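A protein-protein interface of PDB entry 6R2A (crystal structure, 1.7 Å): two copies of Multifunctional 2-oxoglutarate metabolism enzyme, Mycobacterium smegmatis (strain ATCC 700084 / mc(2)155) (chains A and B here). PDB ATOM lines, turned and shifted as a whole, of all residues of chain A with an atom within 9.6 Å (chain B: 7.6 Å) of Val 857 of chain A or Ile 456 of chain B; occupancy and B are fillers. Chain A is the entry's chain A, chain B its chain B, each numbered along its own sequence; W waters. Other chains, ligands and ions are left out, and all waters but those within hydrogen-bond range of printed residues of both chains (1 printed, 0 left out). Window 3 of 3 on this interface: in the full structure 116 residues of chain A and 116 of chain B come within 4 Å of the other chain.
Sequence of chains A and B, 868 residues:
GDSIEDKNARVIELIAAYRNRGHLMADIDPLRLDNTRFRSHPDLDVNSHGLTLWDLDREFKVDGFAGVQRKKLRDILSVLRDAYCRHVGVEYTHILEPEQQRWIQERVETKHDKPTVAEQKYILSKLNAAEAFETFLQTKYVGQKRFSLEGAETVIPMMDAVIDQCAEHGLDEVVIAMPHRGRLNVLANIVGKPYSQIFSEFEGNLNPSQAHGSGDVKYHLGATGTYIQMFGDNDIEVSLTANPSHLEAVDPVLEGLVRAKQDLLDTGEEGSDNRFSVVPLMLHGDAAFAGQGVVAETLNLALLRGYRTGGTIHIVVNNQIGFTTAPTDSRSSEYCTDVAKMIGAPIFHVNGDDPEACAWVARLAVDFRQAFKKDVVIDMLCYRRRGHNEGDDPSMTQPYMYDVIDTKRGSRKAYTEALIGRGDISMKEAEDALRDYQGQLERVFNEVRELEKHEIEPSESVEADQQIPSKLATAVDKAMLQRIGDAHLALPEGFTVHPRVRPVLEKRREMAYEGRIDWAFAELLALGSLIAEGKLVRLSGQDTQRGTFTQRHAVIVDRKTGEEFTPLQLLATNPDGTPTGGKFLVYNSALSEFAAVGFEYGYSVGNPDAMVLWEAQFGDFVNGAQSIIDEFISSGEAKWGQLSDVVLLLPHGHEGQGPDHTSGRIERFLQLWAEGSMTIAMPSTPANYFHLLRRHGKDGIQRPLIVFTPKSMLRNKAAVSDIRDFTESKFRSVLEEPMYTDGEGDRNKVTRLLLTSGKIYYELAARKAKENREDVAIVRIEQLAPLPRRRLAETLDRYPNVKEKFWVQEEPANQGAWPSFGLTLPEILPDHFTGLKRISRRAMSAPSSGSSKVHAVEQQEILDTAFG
The side-chain carboxylate (OE2) of Glu 858 of chain A is in hydrogen-bond range of the backbone NH (N) of Ser 459 of chain B (3.1 Å).
O of Gly 204 of chain B sits at hydrogen-bond distance from NZ of Lys 853 of chain A (3.4 Å).
The backbone carbonyl oxygen (O) of Glu 861 of chain A is in hydrogen-bond range of the side-chain hydroxyl (OG1) of Thr 865 of chain A, at 2.8 Å.
OG of Ser 851 of chain A lies within hydrogen-bond range of N of Lys 853 of chain A, at 3.2 Å.
The side-chain hydroxyl (OG) of Ser 851 of chain A is in hydrogen-bond range of the backbone NH (N) of Val 854 of chain A, at 3.2 Å.
The side-chain carboxylate of Glu 858 of chain A is in salt-bridge range of the guanidinium group of Arg 841 of chain A.
Among the printed residues, merely in contact across the chains: Lys 853 of chain A with Ile 456 of chain B (3.6 Å), Val 854 of chain A with Ile 456 of chain B (3.7 Å), Val 854 of chain A with Glu 457 of chain B (3.7 Å), Val 854 of chain A with Ser 459 of chain B (3.5 Å), Val 857 of chain A with Ile 456 of chain B (3.8 Å), Val 857 of chain A with Pro 458 of chain B (3.98 Å), Glu 858 of chain A with Pro 458 of chain B (3.7 Å) and Glu 861 of chain A with Pro 458 of chain B (3.5 Å).
No residue of chain B comes within 4 Å of Ala 856 of chain A.
Val 857 of chain A touches two residues of chain B.
Of the printed residues of chain B, Glu 861 of chain A touches Pro 458.
Of chain A, only Lys 853, Val 854 and Val 857 come within 4 Å of Ile 456 of chain B.
Printed residues of chain A within 4 Å of Glu 457 of chain B: Val 854.
The nearest residue of chain B that does not touch Val 857 of chain A is Glu 457 of chain B (4.5 Å).
Of the 19 printed residues of chain A, 5 touch a printed residue of chain B.
Of the 10 printed residues of chain B, 5 touch a printed residue of chain A.
Among the printed residues, 10 pairs touch across the chains.
No position is printed for both chains.
Of the 10 pairs that touch across the chains among the printed residues, none has its exchanged pair printed and touching as well.
Water W1 lies within hydrogen-bond range of the side-chain carboxylate of Glu 858 of chain A (2.7 Å) and the side-chain hydroxyl of Ser 459 of chain B (3.5 Å).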
ATOM      1  N   GLY A 656     -12.068   1.598   8.031  1.00  0.00           N
ATOM      2  CA  GLY A 656     -12.608   0.618   8.974  1.00  0.00           C
ATOM      3  C   GLY A 656     -13.876   1.062   9.675  1.00  0.00           C
ATOM      4  O   GLY A 656     -14.272   0.441  10.670  1.00  0.00           O
ATOM      5  N   SER A 840      -6.439  -4.860  -5.596  1.00  0.00           N
ATOM      6  CA  SER A 840      -7.539  -4.222  -4.854  1.00  0.00           C
ATOM      7  C   SER A 840      -8.174  -5.180  -3.872  1.00  0.00           C
ATOM      8  O   SER A 840      -7.769  -6.334  -3.784  1.00  0.00           O
ATOM      9  CB  SER A 840      -8.622  -3.760  -5.834  1.00  0.00           C
ATOM     10  OG  SER A 840      -9.312  -4.871  -6.390  1.00  0.00           O
ATOM     11  N   ARG A 841      -9.242  -4.721  -3.194  1.00  0.00           N
ATOM     12  CA  ARG A 841     -10.065  -5.619  -2.398  1.00  0.00           C
ATOM     13  C   ARG A 841     -10.863  -6.469  -3.395  1.00  0.00           C
ATOM     14  O   ARG A 841     -11.014  -6.059  -4.554  1.00  0.00           O
ATOM     15  CB  ARG A 841     -11.013  -4.825  -1.473  1.00  0.00           C
ATOM     16  CG  ARG A 841     -10.412  -4.541  -0.106  1.00  0.00           C
ATOM     17  CD  ARG A 841     -11.317  -3.672   0.778  1.00  0.00           C
ATOM     18  NE  ARG A 841     -10.698  -3.469   2.094  1.00  0.00           N
ATOM     19  CZ  ARG A 841      -9.745  -2.577   2.362  1.00  0.00           C
ATOM     20  NH1 ARG A 841      -9.210  -2.514   3.576  1.00  0.00           N
ATOM     21  NH2 ARG A 841      -9.316  -1.744   1.417  1.00  0.00           N
ATOM     22  N   SER A 849     -16.210  -3.911   4.479  1.00  0.00           N
ATOM     23  CA  SER A 849     -16.592  -4.769   5.591  1.00  0.00           C
ATOM     24  C   SER A 849     -17.169  -3.889   6.700  1.00  0.00           C
ATOM     25  O   SER A 849     -16.853  -2.695   6.759  1.00  0.00           O
ATOM     26  CB  SER A 849     -15.373  -5.531   6.104  1.00  0.00           C
ATOM     27  OG  SER A 849     -15.538  -5.908   7.460  1.00  0.00           O
ATOM     28  N   SER A 851     -16.496  -4.496   9.877  1.00  0.00           N
ATOM     29  CA  SER A 851     -15.557  -4.599  10.998  1.00  0.00           C
ATOM     30  C   SER A 851     -14.237  -3.859  10.749  1.00  0.00           C
ATOM     31  O   SER A 851     -13.601  -4.083   9.720  1.00  0.00           O
ATOM     32  CB  SER A 851     -15.273  -6.075  11.280  1.00  0.00           C
ATOM     33  OG  SER A 851     -14.083  -6.251  12.030  1.00  0.00           O
ATOM     34  N   SER A 852     -13.793  -3.032  11.725  1.00  0.00           N
ATOM     35  CA  SER A 852     -12.514  -2.317  11.601  1.00  0.00           C
ATOM     36  C   SER A 852     -11.339  -3.305  11.579  1.00  0.00           C
ATOM     37  O   SER A 852     -10.376  -3.074  10.854  1.00  0.00           O
ATOM     38  CB  SER A 852     -12.328  -1.309  12.731  1.00  0.00           C
ATOM     39  OG  SER A 852     -12.405  -1.973  13.981  1.00  0.00           O
ATOM     40  N   LYS A 853     -11.424  -4.421  12.340  1.00  0.00           N
ATOM     41  CA  LYS A 853     -10.354  -5.422  12.354  1.00  0.00           C
ATOM     42  C   LYS A 853     -10.246  -6.116  10.986  1.00  0.00           C
ATOM     43  O   LYS A 853      -9.131  -6.323  10.491  1.00  0.00           O
ATOM     44  CB  LYS A 853     -10.561  -6.445  13.480  1.00  0.00           C
ATOM     45  CG  LYS A 853     -10.346  -5.844  14.870  1.00  0.00           C
ATOM     46  CD  LYS A 853     -10.574  -6.856  15.983  1.00  0.00           C
ATOM     47  CE  LYS A 853     -10.346  -6.234  17.340  1.00  0.00           C
ATOM     48  NZ  LYS A 853     -10.549  -7.214  18.435  1.00  0.00           N
ATOM     49  N   VAL A 854     -11.394  -6.428  10.359  1.00  0.00           N
ATOM     50  CA  VAL A 854     -11.435  -7.078   9.038  1.00  0.00           C
ATOM     51  C   VAL A 854     -10.869  -6.097   7.981  1.00  0.00           C
ATOM     52  O   VAL A 854     -10.041  -6.498   7.156  1.00  0.00           O
ATOM     53  CB  VAL A 854     -12.858  -7.596   8.687  1.00  0.00           C
ATOM     54  CG1 VAL A 854     -12.922  -8.102   7.249  1.00  0.00           C
ATOM     55  CG2 VAL A 854     -13.284  -8.703   9.656  1.00  0.00           C
ATOM     56  N   HIS A 855     -11.262  -4.806   8.059  1.00  0.00           N
ATOM     57  CA  HIS A 855     -10.719  -3.776   7.174  1.00  0.00           C
ATOM     58  C   HIS A 855      -9.182  -3.773   7.219  1.00  0.00           C
ATOM     59  O   HIS A 855      -8.536  -3.725   6.171  1.00  0.00           O
ATOM     60  CB  HIS A 855     -11.232  -2.388   7.590  1.00  0.00           C
ATOM     61  CG  HIS A 855     -10.294  -1.276   7.216  1.00  0.00           C
ATOM     62  ND1 HIS A 855     -10.187  -0.830   5.911  1.00  0.00           N
ATOM     63  CD2 HIS A 855      -9.403  -0.598   7.981  1.00  0.00           C
ATOM     64  CE1 HIS A 855      -9.258   0.115   5.926  1.00  0.00           C
ATOM     65  NE2 HIS A 855      -8.753   0.284   7.150  1.00  0.00           N
ATOM     66  N   ALA A 856      -8.610  -3.783   8.445  1.00  0.00           N
ATOM     67  CA  ALA A 856      -7.171  -3.706   8.663  1.00  0.00           C
ATOM     68  C   ALA A 856      -6.412  -4.878   8.010  1.00  0.00           C
ATOM     69  O   ALA A 856      -5.375  -4.641   7.392  1.00  0.00           O
ATOM     70  CB  ALA A 856      -6.867  -3.644  10.150  1.00  0.00           C
ATOM     71  N   VAL A 857      -6.947  -6.113   8.103  1.00  0.00           N
ATOM     72  CA  VAL A 857      -6.310  -7.310   7.524  1.00  0.00           C
ATOM     73  C   VAL A 857      -6.351  -7.197   5.993  1.00  0.00           C
ATOM     74  O   VAL A 857      -5.341  -7.468   5.334  1.00  0.00           O
ATOM     75  CB  VAL A 857      -6.959  -8.621   8.047  1.00  0.00           C
ATOM     76  CG1 VAL A 857      -6.475  -9.842   7.267  1.00  0.00           C
ATOM     77  CG2 VAL A 857      -6.684  -8.798   9.541  1.00  0.00           C
ATOM     78  N   GLU A 858      -7.502  -6.764   5.442  1.00  0.00           N
ATOM     79  CA  GLU A 858      -7.669  -6.564   4.001  1.00  0.00           C
ATOM     80  C   GLU A 858      -6.733  -5.477   3.480  1.00  0.00           C
ATOM     81  O   GLU A 858      -6.165  -5.637   2.397  1.00  0.00           O
ATOM     82  CB  GLU A 858      -9.114  -6.190   3.668  1.00  0.00           C
ATOM     83  CG  GLU A 858     -10.123  -7.295   3.920  1.00  0.00           C
ATOM     84  CD  GLU A 858     -11.559  -6.822   3.779  1.00  0.00           C
ATOM     85  OE1 GLU A 858     -11.773  -5.600   3.595  1.00  0.00           O
ATOM     86  OE2 GLU A 858     -12.473  -7.673   3.870  1.00  0.00           O
ATOM     87  N   GLN A 859      -6.560  -4.381   4.249  1.00  0.00           N
ATOM     88  CA  GLN A 859      -5.677  -3.274   3.857  1.00  0.00           C
ATOM     89  C   GLN A 859      -4.227  -3.749   3.755  1.00  0.00           C
ATOM     90  O   GLN A 859      -3.535  -3.423   2.784  1.00  0.00           O
ATOM     91  CB  GLN A 859      -5.775  -2.107   4.849  1.00  0.00           C
ATOM     92  CG  GLN A 859      -5.156  -0.798   4.321  1.00  0.00           C
ATOM     93  CD  GLN A 859      -6.073  -0.013   3.386  1.00  0.00           C
ATOM     94  OE1 GLN A 859      -7.163  -0.450   3.013  1.00  0.00           O
ATOM     95  NE2 GLN A 859      -5.644   1.175   2.985  1.00  0.00           N
ATOM     96  N   GLN A 860      -3.774  -4.526   4.755  1.00  0.00           N
ATOM     97  CA  GLN A 860      -2.417  -5.065   4.790  1.00  0.00           C
ATOM     98  C   GLN A 860      -2.173  -6.014   3.600  1.00  0.00           C
ATOM     99  O   GLN A 860      -1.068  -6.004   3.058  1.00  0.00           O
ATOM    100  CB  GLN A 860      -2.142  -5.766   6.131  1.00  0.00           C
ATOM    101  CG  GLN A 860      -0.653  -5.973   6.450  1.00  0.00           C
ATOM    102  CD  GLN A 860       0.206  -4.749   6.228  1.00  0.00           C
ATOM    103  OE1 GLN A 860       1.004  -4.714   5.293  1.00  0.00           O
ATOM    104  NE2 GLN A 860       0.065  -3.714   7.055  1.00  0.00           N
ATOM    105  N   GLU A 861      -3.200  -6.791   3.173  1.00  0.00           N
ATOM    106  CA  GLU A 861      -3.102  -7.700   2.015  1.00  0.00           C
ATOM    107  C   GLU A 861      -2.766  -6.935   0.733  1.00  0.00           C
ATOM    108  O   GLU A 861      -1.949  -7.408  -0.051  1.00  0.00           O
ATOM    109  CB  GLU A 861      -4.408  -8.474   1.791  1.00  0.00           C
ATOM    110  CG  GLU A 861      -4.572  -9.721   2.638  1.00  0.00           C
ATOM    111  CD  GLU A 861      -5.735 -10.618   2.250  1.00  0.00           C
ATOM    112  OE1 GLU A 861      -5.650 -11.837   2.521  1.00  0.00           O
ATOM    113  OE2 GLU A 861      -6.735 -10.112   1.689  1.00  0.00           O
ATOM    114  N   ILE A 862      -3.397  -5.765   0.520  1.00  0.00           N
ATOM    115  CA  ILE A 862      -3.158  -4.918  -0.657  1.00  0.00           C
ATOM    116  C   ILE A 862      -1.695  -4.453  -0.667  1.00  0.00           C
ATOM    117  O   ILE A 862      -1.024  -4.560  -1.699  1.00  0.00           O
ATOM    118  CB  ILE A 862      -4.130  -3.708  -0.689  1.00  0.00           C
ATOM    119  CG1 ILE A 862      -5.594  -4.176  -0.895  1.00  0.00           C
ATOM    120  CG2 ILE A 862      -3.711  -2.696  -1.762  1.00  0.00           C
ATOM    121  CD1 ILE A 862      -6.649  -3.099  -0.600  1.00  0.00           C
ATOM    122  N   LEU A 863      -1.211  -3.942   0.485  1.00  0.00           N
ATOM    123  CA  LEU A 863       0.163  -3.446   0.623  1.00  0.00           C
ATOM    124  C   LEU A 863       1.173  -4.580   0.392  1.00  0.00           C
ATOM    125  O   LEU A 863       2.142  -4.385  -0.348  1.00  0.00           O
ATOM    126  CB  LEU A 863       0.391  -2.770   1.989  1.00  0.00           C
ATOM    127  CG  LEU A 863      -0.530  -1.593   2.375  1.00  0.00           C
ATOM    128  CD1 LEU A 863      -0.088  -0.978   3.691  1.00  0.00           C
ATOM    129  CD2 LEU A 863      -0.583  -0.511   1.289  1.00  0.00           C
ATOM    130  N   ASP A 864       0.910  -5.770   0.966  1.00  0.00           N
ATOM    131  CA  ASP A 864       1.770  -6.943   0.802  1.00  0.00           C
ATOM    132  C   ASP A 864       1.804  -7.414  -0.659  1.00  0.00           C
ATOM    133  O   ASP A 864       2.882  -7.764  -1.145  1.00  0.00           O
ATOM    134  CB  ASP A 864       1.330  -8.095   1.724  1.00  0.00           C
ATOM    135  CG  ASP A 864       1.562  -7.847   3.208  1.00  0.00           C
ATOM    136  OD1 ASP A 864       2.254  -6.858   3.550  1.00  0.00           O
ATOM    137  OD2 ASP A 864       1.046  -8.635   4.027  1.00  0.00           O
ATOM    138  N   THR A 865       0.647  -7.396  -1.359  1.00  0.00           N
ATOM    139  CA  THR A 865       0.543  -7.800  -2.766  1.00  0.00           C
ATOM    140  C   THR A 865       1.312  -6.816  -3.661  1.00  0.00           C
ATOM    141  O   THR A 865       2.013  -7.259  -4.569  1.00  0.00           O
ATOM    142  CB  THR A 865      -0.937  -7.928  -3.183  1.00  0.00           C
ATOM    143  OG1 THR A 865      -1.548  -8.914  -2.353  1.00  0.00           O
ATOM    144  CG2 THR A 865      -1.118  -8.333  -4.646  1.00  0.00           C
ATOM    145  N   GLY B 204     -14.677  -7.149  19.475  1.00  0.00           N
ATOM    146  CA  GLY B 204     -14.223  -7.504  18.137  1.00  0.00           C
ATOM    147  C   GLY B 204     -13.856  -8.970  18.077  1.00  0.00           C
ATOM    148  O   GLY B 204     -12.988  -9.367  17.299  1.00  0.00           O
ATOM    149  N   ASN B 205     -14.495  -9.775  18.937  1.00  0.00           N
ATOM    150  CA  ASN B 205     -14.290 -11.212  19.018  1.00  0.00           C
ATOM    151  C   ASN B 205     -15.583 -11.893  18.573  1.00  0.00           C
ATOM    152  O   ASN B 205     -16.475 -12.155  19.386  1.00  0.00           O
ATOM    153  CB  ASN B 205     -13.864 -11.618  20.434  1.00  0.00           C
ATOM    154  CG  ASN B 205     -13.431 -13.057  20.545  1.00  0.00           C
ATOM    155  OD1 ASN B 205     -12.910 -13.658  19.593  1.00  0.00           O
ATOM    156  ND2 ASN B 205     -13.640 -13.637  21.716  1.00  0.00           N
ATOM    157  N   LEU B 206     -15.704 -12.104  17.254  1.00  0.00           N
ATOM    158  CA  LEU B 206     -16.891 -12.690  16.637  1.00  0.00           C
ATOM    159  C   LEU B 206     -16.670 -14.147  16.246  1.00  0.00           C
ATOM    160  O   LEU B 206     -15.623 -14.489  15.688  1.00  0.00           O
ATOM    161  CB  LEU B 206     -17.311 -11.878  15.385  1.00  0.00           C
ATOM    162  CG  LEU B 206     -17.809 -10.411  15.537  1.00  0.00           C
ATOM    163  CD1 LEU B 206     -18.616 -10.176  16.821  1.00  0.00           C
ATOM    164  CD2 LEU B 206     -16.675  -9.417  15.398  1.00  0.00           C
ATOM    165  N   LYS B 453     -10.088 -15.900  21.751  1.00  0.00           N
ATOM    166  CA  LYS B 453     -10.014 -14.966  20.628  1.00  0.00           C
ATOM    167  C   LYS B 453      -9.832 -15.727  19.318  1.00  0.00           C
ATOM    168  O   LYS B 453      -9.048 -16.677  19.264  1.00  0.00           O
ATOM    169  CB  LYS B 453      -8.878 -13.954  20.825  1.00  0.00           C
ATOM    170  N   HIS B 454     -10.585 -15.319  18.279  1.00  0.00           N
ATOM    171  CA  HIS B 454     -10.566 -15.881  16.920  1.00  0.00           C
ATOM    172  C   HIS B 454      -9.638 -15.069  16.009  1.00  0.00           C
ATOM    173  O   HIS B 454      -9.573 -13.843  16.161  1.00  0.00           O
ATOM    174  CB  HIS B 454     -11.985 -15.873  16.307  1.00  0.00           C
ATOM    175  CG  HIS B 454     -13.022 -16.607  17.102  1.00  0.00           C
ATOM    176  ND1 HIS B 454     -13.109 -17.989  17.074  1.00  0.00           N
ATOM    177  CD2 HIS B 454     -14.010 -16.123  17.890  1.00  0.00           C
ATOM    178  CE1 HIS B 454     -14.127 -18.300  17.862  1.00  0.00           C
ATOM    179  NE2 HIS B 454     -14.701 -17.210  18.375  1.00  0.00           N
ATOM    180  N   GLU B 455      -8.954 -15.735  15.043  1.00  0.00           N
ATOM    181  CA  GLU B 455      -8.097 -15.048  14.068  1.00  0.00           C
ATOM    182  C   GLU B 455      -8.976 -14.213  13.149  1.00  0.00           C
ATOM    183  O   GLU B 455     -10.073 -14.655  12.791  1.00  0.00           O
ATOM    184  CB  GLU B 455      -7.270 -16.052  13.251  1.00  0.00           C
ATOM    185  N   ILE B 456      -8.528 -13.001  12.807  1.00  0.00           N
ATOM    186  CA  ILE B 456      -9.291 -12.106  11.938  1.00  0.00           C
ATOM    187  C   ILE B 456      -8.911 -12.415  10.491  1.00  0.00           C
ATOM    188  O   ILE B 456      -7.734 -12.412  10.143  1.00  0.00           O
ATOM    189  CB  ILE B 456      -9.105 -10.605  12.301  1.00  0.00           C
ATOM    190  CG1 ILE B 456      -9.478 -10.337  13.765  1.00  0.00           C
ATOM    191  CG2 ILE B 456      -9.925  -9.689  11.378  1.00  0.00           C
ATOM    192  CD1 ILE B 456      -8.426  -9.740  14.484  1.00  0.00           C
ATOM    193  N   GLU B 457      -9.917 -12.673   9.658  1.00  0.00           N
ATOM    194  CA  GLU B 457      -9.729 -12.988   8.245  1.00  0.00           C
ATOM    195  C   GLU B 457     -10.447 -11.971   7.356  1.00  0.00           C
ATOM    196  O   GLU B 457     -11.462 -11.407   7.786  1.00  0.00           O
ATOM    197  CB  GLU B 457     -10.289 -14.397   7.940  1.00  0.00           C
ATOM    198  CG  GLU B 457      -9.574 -15.540   8.648  1.00  0.00           C
ATOM    199  CD  GLU B 457     -10.148 -16.922   8.399  1.00  0.00           C
ATOM    200  OE1 GLU B 457     -11.393 -17.065   8.366  1.00  0.00           O
ATOM    201  OE2 GLU B 457      -9.345 -17.870   8.247  1.00  0.00           O
ATOM    202  N   PRO B 458     -10.021 -11.792   6.079  1.00  0.00           N
ATOM    203  CA  PRO B 458     -10.801 -10.929   5.170  1.00  0.00           C
ATOM    204  C   PRO B 458     -12.227 -11.468   5.026  1.00  0.00           C
ATOM    205  O   PRO B 458     -12.438 -12.683   5.142  1.00  0.00           O
ATOM    206  CB  PRO B 458     -10.045 -11.039   3.840  1.00  0.00           C
ATOM    207  CG  PRO B 458      -8.681 -11.502   4.199  1.00  0.00           C
ATOM    208  CD  PRO B 458      -8.868 -12.400   5.383  1.00  0.00           C
ATOM    209  N   SER B 459     -13.210 -10.582   4.810  1.00  0.00           N
ATOM    210  CA  SER B 459     -14.594 -11.016   4.642  1.00  0.00           C
ATOM    211  C   SER B 459     -14.728 -11.893   3.388  1.00  0.00           C
ATOM    212  O   SER B 459     -13.907 -11.788   2.466  1.00  0.00           O
ATOM    213  CB  SER B 459     -15.530  -9.813   4.562  1.00  0.00           C
ATOM    214  OG  SER B 459     -15.345  -9.098   3.352  1.00  0.00           O
HETATM  215  O   HOH W   1     -12.951  -7.801   1.190  1.00  0.00           O
